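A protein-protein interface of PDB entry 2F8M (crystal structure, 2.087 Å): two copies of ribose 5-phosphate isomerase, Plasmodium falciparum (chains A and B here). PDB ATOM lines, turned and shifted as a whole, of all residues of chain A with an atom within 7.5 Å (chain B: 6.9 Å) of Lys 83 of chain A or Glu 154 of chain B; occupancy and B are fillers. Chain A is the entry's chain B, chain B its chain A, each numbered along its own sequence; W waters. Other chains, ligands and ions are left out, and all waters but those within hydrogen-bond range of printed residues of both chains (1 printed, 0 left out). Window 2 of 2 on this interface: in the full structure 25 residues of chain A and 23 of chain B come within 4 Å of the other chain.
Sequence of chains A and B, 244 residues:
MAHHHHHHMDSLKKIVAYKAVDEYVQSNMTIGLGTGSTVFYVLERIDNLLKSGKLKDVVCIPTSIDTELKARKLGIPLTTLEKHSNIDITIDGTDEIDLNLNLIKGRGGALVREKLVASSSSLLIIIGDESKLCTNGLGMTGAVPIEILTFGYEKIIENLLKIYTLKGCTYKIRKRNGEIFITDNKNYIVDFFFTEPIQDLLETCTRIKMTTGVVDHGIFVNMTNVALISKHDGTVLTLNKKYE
O of Leu 81 of chain A touches CA of Gly 152 of chain B (3.5 Å).
CB of Lys 155 of chain B touches CG of Leu 81 of chain A (3.7 Å).
Glu 82 of chain A touches Lys 155 of chain B.
Lys 83 of chain A touches Glu 154 of chain B.
Glu 158 of chain B touches Lys 83 of chain A (CB to O, 3.4 Å).
Leu 116 of chain A touches Phe 151 of chain B.
O of Lys 83 of chain A sits close to NZ of Lys 155 of chain B (3.5 Å).
The side-chain amino group (NZ) of Lys 155 of chain B lies within hydrogen-bond range of the backbone carbonyl oxygen (O) of Ser 85 of chain A (2.9 Å).
No position is printed for both chains.
Of the 8 pairs that touch across the chains among the printed residues, none has its exchanged pair printed and touching as well.
The side-chain hydroxyl of Thr 80 of chain A sits at hydrogen-bond distance from the side-chain carboxylate of Glu 82 of chain A, at 3.5 Å.
N of Glu 82 of chain A is in hydrogen-bond range of OG of Ser 85 of chain A, at 2.8 Å.
Water W1 lies within hydrogen-bond range of O of Leu 81 of chain A (2.8 Å), N of Glu 154 of chain B (3.1 Å) and N of Tyr 153 of chain B (3.3 Å).
Of the printed residues of chain B, Glu 82 of chain A touches Lys 155.
Lys 83 of chain A touches three residues of chain B.
Printed residues of chain B within 4 Å of Ser 85 of chain A: Lys 155.
Of the printed residues of chain B, Leu 116 of chain A touches Phe 151 (3.8 Å).
Of chain A, only Lys 83 comes within 4 Å of Glu 154 of chain B.
Tyr 171 of chain B touches none of the printed residues of chain A.
The nearest residue of chain A that does not touch Glu 154 of chain B is Glu 82 of chain A (4.2 Å).
Hydrophobic or aromatic side chains of chain A within 4 Å of the printed part of chain B: Leu 81 and Leu 116.
Among the printed residues, 8 pairs touch across the chains.
Among the printed residues, no Asp or Glu carboxylate lies within 4 Å of a Lys or Arg side-chain nitrogen of the other chain.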
ATOM      1  N   THR A  80       6.540  24.448   1.475  1.00  0.00           N
ATOM      2  CA  THR A  80       7.143  23.372   2.185  1.00  0.00           C
ATOM      3  C   THR A  80       6.741  23.454   3.646  1.00  0.00           C
ATOM      4  O   THR A  80       6.307  24.503   4.160  1.00  0.00           O
ATOM      5  CB  THR A  80       8.659  23.422   2.050  1.00  0.00           C
ATOM      6  OG1 THR A  80       9.159  24.636   2.642  1.00  0.00           O
ATOM      7  CG2 THR A  80       9.062  23.346   0.556  1.00  0.00           C
ATOM      8  N   LEU A  81       6.912  22.319   4.297  1.00  0.00           N
ATOM      9  CA  LEU A  81       6.607  22.172   5.691  1.00  0.00           C
ATOM     10  C   LEU A  81       7.758  22.786   6.535  1.00  0.00           C
ATOM     11  O   LEU A  81       8.808  22.165   6.697  1.00  0.00           O
ATOM     12  CB  LEU A  81       6.352  20.692   5.974  1.00  0.00           C
ATOM     13  CG  LEU A  81       5.747  20.350   7.337  1.00  0.00           C
ATOM     14  CD1 LEU A  81       4.363  21.027   7.599  1.00  0.00           C
ATOM     15  CD2 LEU A  81       5.636  18.840   7.468  1.00  0.00           C
ATOM     16  N   GLU A  82       7.527  24.017   7.026  1.00  0.00           N
ATOM     17  CA  GLU A  82       8.510  24.863   7.727  1.00  0.00           C
ATOM     18  C   GLU A  82       8.267  24.863   9.257  1.00  0.00           C
ATOM     19  O   GLU A  82       7.274  24.309   9.729  1.00  0.00           O
ATOM     20  CB  GLU A  82       8.464  26.306   7.153  1.00  0.00           C
ATOM     21  CG  GLU A  82       8.935  26.476   5.649  1.00  0.00           C
ATOM     22  CD  GLU A  82       8.438  27.809   4.957  1.00  0.00           C
ATOM     23  OE1 GLU A  82       8.115  28.789   5.696  1.00  0.00           O
ATOM     24  OE2 GLU A  82       8.360  27.878   3.677  1.00  0.00           O
ATOM     25  N   LYS A  83       9.157  25.498  10.026  1.00  0.00           N
ATOM     26  CA  LYS A  83       9.168  25.393  11.515  1.00  0.00           C
ATOM     27  C   LYS A  83       7.779  25.402  12.189  1.00  0.00           C
ATOM     28  O   LYS A  83       7.390  24.436  12.872  1.00  0.00           O
ATOM     29  CB  LYS A  83      10.052  26.493  12.151  1.00  0.00           C
ATOM     30  N   HIS A  84       7.032  26.489  12.049  1.00  0.00           N
ATOM     31  CA  HIS A  84       5.639  26.466  12.545  1.00  0.00           C
ATOM     32  C   HIS A  84       4.634  26.687  11.400  1.00  0.00           C
ATOM     33  O   HIS A  84       3.838  27.629  11.418  1.00  0.00           O
ATOM     34  CB  HIS A  84       5.393  27.435  13.733  1.00  0.00           C
ATOM     35  CG  HIS A  84       6.234  28.677  13.708  1.00  0.00           C
ATOM     36  ND1 HIS A  84       6.706  29.274  14.862  1.00  0.00           N
ATOM     37  CD2 HIS A  84       6.702  29.424  12.674  1.00  0.00           C
ATOM     38  CE1 HIS A  84       7.422  30.339  14.537  1.00  0.00           C
ATOM     39  NE2 HIS A  84       7.446  30.447  13.217  1.00  0.00           N
ATOM     40  N   SER A  85       4.689  25.803  10.411  1.00  0.00           N
ATOM     41  CA  SER A  85       3.541  25.579   9.559  1.00  0.00           C
ATOM     42  C   SER A  85       2.414  24.944  10.376  1.00  0.00           C
ATOM     43  O   SER A  85       2.656  24.024  11.181  1.00  0.00           O
ATOM     44  CB  SER A  85       3.895  24.661   8.382  1.00  0.00           C
ATOM     45  OG  SER A  85       5.035  25.126   7.710  1.00  0.00           O
ATOM     46  N   ASN A  86       1.188  25.445  10.172  1.00  0.00           N
ATOM     47  CA  ASN A  86      -0.003  24.655  10.451  1.00  0.00           C
ATOM     48  C   ASN A  86      -0.757  24.383   9.162  1.00  0.00           C
ATOM     49  O   ASN A  86      -1.114  25.290   8.430  1.00  0.00           O
ATOM     50  CB  ASN A  86      -0.956  25.331  11.450  1.00  0.00           C
ATOM     51  CG  ASN A  86      -2.061  24.377  11.940  1.00  0.00           C
ATOM     52  OD1 ASN A  86      -3.243  24.499  11.575  1.00  0.00           O
ATOM     53  ND2 ASN A  86      -1.667  23.409  12.738  1.00  0.00           N
ATOM     54  N   LEU A 116       3.719  12.763   8.170  1.00  0.00           N
ATOM     55  CA  LEU A 116       4.249  13.985   8.737  1.00  0.00           C
ATOM     56  C   LEU A 116       3.351  15.180   8.376  1.00  0.00           C
ATOM     57  O   LEU A 116       3.012  15.996   9.243  1.00  0.00           O
ATOM     58  CB  LEU A 116       5.661  14.213   8.224  1.00  0.00           C
ATOM     59  CG  LEU A 116       6.245  15.548   8.665  1.00  0.00           C
ATOM     60  CD1 LEU A 116       6.213  15.697  10.181  1.00  0.00           C
ATOM     61  CD2 LEU A 116       7.676  15.750   8.117  1.00  0.00           C
ATOM     62  N   ILE B 148      17.301  12.930  10.746  1.00  0.00           N
ATOM     63  CA  ILE B 148      15.915  13.302  10.403  1.00  0.00           C
ATOM     64  C   ILE B 148      15.819  13.398   8.939  1.00  0.00           C
ATOM     65  O   ILE B 148      16.835  13.607   8.271  1.00  0.00           O
ATOM     66  CB  ILE B 148      15.503  14.687  11.018  1.00  0.00           C
ATOM     67  CG1 ILE B 148      16.455  15.793  10.534  1.00  0.00           C
ATOM     68  CG2 ILE B 148      15.469  14.586  12.554  1.00  0.00           C
ATOM     69  CD1 ILE B 148      16.191  17.199  11.036  1.00  0.00           C
ATOM     70  N   LEU B 149      14.594  13.285   8.427  1.00  0.00           N
ATOM     71  CA  LEU B 149      14.357  13.426   7.017  1.00  0.00           C
ATOM     72  C   LEU B 149      14.659  14.833   6.530  1.00  0.00           C
ATOM     73  O   LEU B 149      14.436  15.811   7.212  1.00  0.00           O
ATOM     74  CB  LEU B 149      12.885  13.145   6.657  1.00  0.00           C
ATOM     75  CG  LEU B 149      12.217  11.861   7.101  1.00  0.00           C
ATOM     76  CD1 LEU B 149      10.768  11.984   6.719  1.00  0.00           C
ATOM     77  CD2 LEU B 149      12.859  10.593   6.495  1.00  0.00           C
ATOM     78  N   THR B 150      15.083  14.906   5.282  1.00  0.00           N
ATOM     79  CA  THR B 150      15.234  16.179   4.589  1.00  0.00           C
ATOM     80  C   THR B 150      13.868  16.824   4.360  1.00  0.00           C
ATOM     81  O   THR B 150      13.693  18.028   4.505  1.00  0.00           O
ATOM     82  CB  THR B 150      15.937  15.953   3.227  1.00  0.00           C
ATOM     83  OG1 THR B 150      15.052  15.259   2.323  1.00  0.00           O
ATOM     84  CG2 THR B 150      17.235  15.137   3.412  1.00  0.00           C
ATOM     85  N   PHE B 151      12.874  16.019   4.014  1.00  0.00           N
ATOM     86  CA  PHE B 151      11.587  16.570   3.787  1.00  0.00           C
ATOM     87  C   PHE B 151      10.979  16.997   5.102  1.00  0.00           C
ATOM     88  O   PHE B 151      10.811  16.156   5.989  1.00  0.00           O
ATOM     89  CB  PHE B 151      10.652  15.572   3.105  1.00  0.00           C
ATOM     90  CG  PHE B 151       9.266  16.104   2.913  1.00  0.00           C
ATOM     91  CD1 PHE B 151       8.941  16.822   1.765  1.00  0.00           C
ATOM     92  CD2 PHE B 151       8.294  15.931   3.902  1.00  0.00           C
ATOM     93  CE1 PHE B 151       7.652  17.287   1.609  1.00  0.00           C
ATOM     94  CE2 PHE B 151       7.017  16.429   3.752  1.00  0.00           C
ATOM     95  CZ  PHE B 151       6.696  17.092   2.618  1.00  0.00           C
ATOM     96  N   GLY B 152      10.673  18.304   5.201  1.00  0.00           N
ATOM     97  CA  GLY B 152      10.087  18.925   6.389  1.00  0.00           C
ATOM     98  C   GLY B 152      10.917  18.985   7.663  1.00  0.00           C
ATOM     99  O   GLY B 152      10.361  19.011   8.753  1.00  0.00           O
ATOM    100  N   TYR B 153      12.234  19.055   7.523  1.00  0.00           N
ATOM    101  CA  TYR B 153      13.163  18.926   8.653  1.00  0.00           C
ATOM    102  C   TYR B 153      13.008  19.994   9.722  1.00  0.00           C
ATOM    103  O   TYR B 153      13.204  19.711  10.906  1.00  0.00           O
ATOM    104  CB  TYR B 153      14.612  18.851   8.150  1.00  0.00           C
ATOM    105  CG  TYR B 153      15.191  20.144   7.661  1.00  0.00           C
ATOM    106  CD1 TYR B 153      14.912  20.624   6.355  1.00  0.00           C
ATOM    107  CD2 TYR B 153      16.030  20.883   8.480  1.00  0.00           C
ATOM    108  CE1 TYR B 153      15.436  21.836   5.898  1.00  0.00           C
ATOM    109  CE2 TYR B 153      16.576  22.078   8.042  1.00  0.00           C
ATOM    110  CZ  TYR B 153      16.280  22.561   6.744  1.00  0.00           C
ATOM    111  OH  TYR B 153      16.827  23.767   6.324  1.00  0.00           O
ATOM    112  N   GLU B 154      12.624  21.200   9.348  1.00  0.00           N
ATOM    113  CA  GLU B 154      12.426  22.241  10.346  1.00  0.00           C
ATOM    114  C   GLU B 154      11.216  21.995  11.183  1.00  0.00           C
ATOM    115  O   GLU B 154      11.194  22.354  12.335  1.00  0.00           O
ATOM    116  CB  GLU B 154      12.271  23.616   9.689  1.00  0.00           C
ATOM    117  CG  GLU B 154      13.417  23.981   8.721  1.00  0.00           C
ATOM    118  CD  GLU B 154      14.417  24.953   9.326  1.00  0.00           C
ATOM    119  OE1 GLU B 154      14.749  24.826  10.545  1.00  0.00           O
ATOM    120  OE2 GLU B 154      14.869  25.853   8.571  1.00  0.00           O
ATOM    121  N   LYS B 155      10.194  21.385  10.605  1.00  0.00           N
ATOM    122  CA  LYS B 155       9.006  21.039  11.347  1.00  0.00           C
ATOM    123  C   LYS B 155       9.357  19.904  12.333  1.00  0.00           C
ATOM    124  O   LYS B 155       8.990  19.924  13.494  1.00  0.00           O
ATOM    125  CB  LYS B 155       7.879  20.658  10.377  1.00  0.00           C
ATOM    126  CG  LYS B 155       6.649  20.062  11.029  1.00  0.00           C
ATOM    127  CD  LYS B 155       6.094  20.919  12.228  1.00  0.00           C
ATOM    128  CE  LYS B 155       5.293  22.112  11.773  1.00  0.00           C
ATOM    129  NZ  LYS B 155       4.428  22.589  12.906  1.00  0.00           N
ATOM    130  N   ILE B 156      10.156  18.959  11.868  1.00  0.00           N
ATOM    131  CA  ILE B 156      10.607  17.848  12.708  1.00  0.00           C
ATOM    132  C   ILE B 156      11.387  18.407  13.874  1.00  0.00           C
ATOM    133  O   ILE B 156      11.164  18.005  15.001  1.00  0.00           O
ATOM    134  CB  ILE B 156      11.467  16.843  11.901  1.00  0.00           C
ATOM    135  CG1 ILE B 156      10.631  16.223  10.778  1.00  0.00           C
ATOM    136  CG2 ILE B 156      11.994  15.753  12.783  1.00  0.00           C
ATOM    137  CD1 ILE B 156      11.440  15.625   9.722  1.00  0.00           C
ATOM    138  N   ILE B 157      12.288  19.349  13.614  1.00  0.00           N
ATOM    139  CA  ILE B 157      13.042  19.968  14.717  1.00  0.00           C
ATOM    140  C   ILE B 157      12.134  20.657  15.757  1.00  0.00           C
ATOM    141  O   ILE B 157      12.330  20.470  16.978  1.00  0.00           O
ATOM    142  CB  ILE B 157      14.110  20.943  14.166  1.00  0.00           C
ATOM    143  CG1 ILE B 157      15.230  20.149  13.537  1.00  0.00           C
ATOM    144  CG2 ILE B 157      14.691  21.794  15.260  1.00  0.00           C
ATOM    145  CD1 ILE B 157      16.014  20.932  12.599  1.00  0.00           C
ATOM    146  N   GLU B 158      11.157  21.457  15.281  1.00  0.00           N
ATOM    147  CA  GLU B 158      10.142  22.091  16.175  1.00  0.00           C
ATOM    148  C   GLU B 158       9.405  21.049  17.022  1.00  0.00           C
ATOM    149  O   GLU B 158       9.112  21.264  18.219  1.00  0.00           O
ATOM    150  CB  GLU B 158       9.123  22.952  15.391  1.00  0.00           C
ATOM    151  N   ASN B 159       9.088  19.917  16.415  1.00  0.00           N
ATOM    152  CA  ASN B 159       8.449  18.853  17.161  1.00  0.00           C
ATOM    153  C   ASN B 159       9.394  18.259  18.184  1.00  0.00           C
ATOM    154  O   ASN B 159       8.972  17.959  19.290  1.00  0.00           O
ATOM    155  CB  ASN B 159       7.867  17.781  16.217  1.00  0.00           C
ATOM    156  CG  ASN B 159       6.632  18.296  15.435  1.00  0.00           C
ATOM    157  OD1 ASN B 159       6.031  19.301  15.814  1.00  0.00           O
ATOM    158  ND2 ASN B 159       6.271  17.619  14.349  1.00  0.00           N
ATOM    159  N   TYR B 171      20.178  24.228  19.023  1.00  0.00           N
ATOM    160  CA  TYR B 171      20.475  23.251  18.030  1.00  0.00           C
ATOM    161  C   TYR B 171      20.912  23.885  16.734  1.00  0.00           C
ATOM    162  O   TYR B 171      20.557  25.017  16.437  1.00  0.00           O
ATOM    163  CB  TYR B 171      19.232  22.430  17.731  1.00  0.00           C
ATOM    164  CG  TYR B 171      18.205  23.293  17.086  1.00  0.00           C
ATOM    165  CD1 TYR B 171      18.214  23.512  15.726  1.00  0.00           C
ATOM    166  CD2 TYR B 171      17.274  23.950  17.860  1.00  0.00           C
ATOM    167  CE1 TYR B 171      17.271  24.369  15.139  1.00  0.00           C
ATOM    168  CE2 TYR B 171      16.349  24.774  17.307  1.00  0.00           C
ATOM    169  CZ  TYR B 171      16.351  24.984  15.953  1.00  0.00           C
ATOM    170  OH  TYR B 171      15.392  25.820  15.445  1.00  0.00           O
ATOM    171  N   ILE B 173      21.307  22.573  12.545  1.00  0.00           N
ATOM    172  CA  ILE B 173      21.406  21.563  11.488  1.00  0.00           C
ATOM    173  C   ILE B 173      22.881  21.362  11.170  1.00  0.00           C
ATOM    174  O   ILE B 173      23.651  22.322  11.161  1.00  0.00           O
ATOM    175  CB  ILE B 173      20.697  21.912  10.182  1.00  0.00           C
ATOM    176  CG1 ILE B 173      20.250  20.643   9.464  1.00  0.00           C
ATOM    177  CG2 ILE B 173      21.635  22.649   9.220  1.00  0.00           C
ATOM    178  CD1 ILE B 173      19.109  19.937  10.127  1.00  0.00           C
HETATM  179  O   HOH W   1      11.592  22.104   6.588  1.00  0.00           O
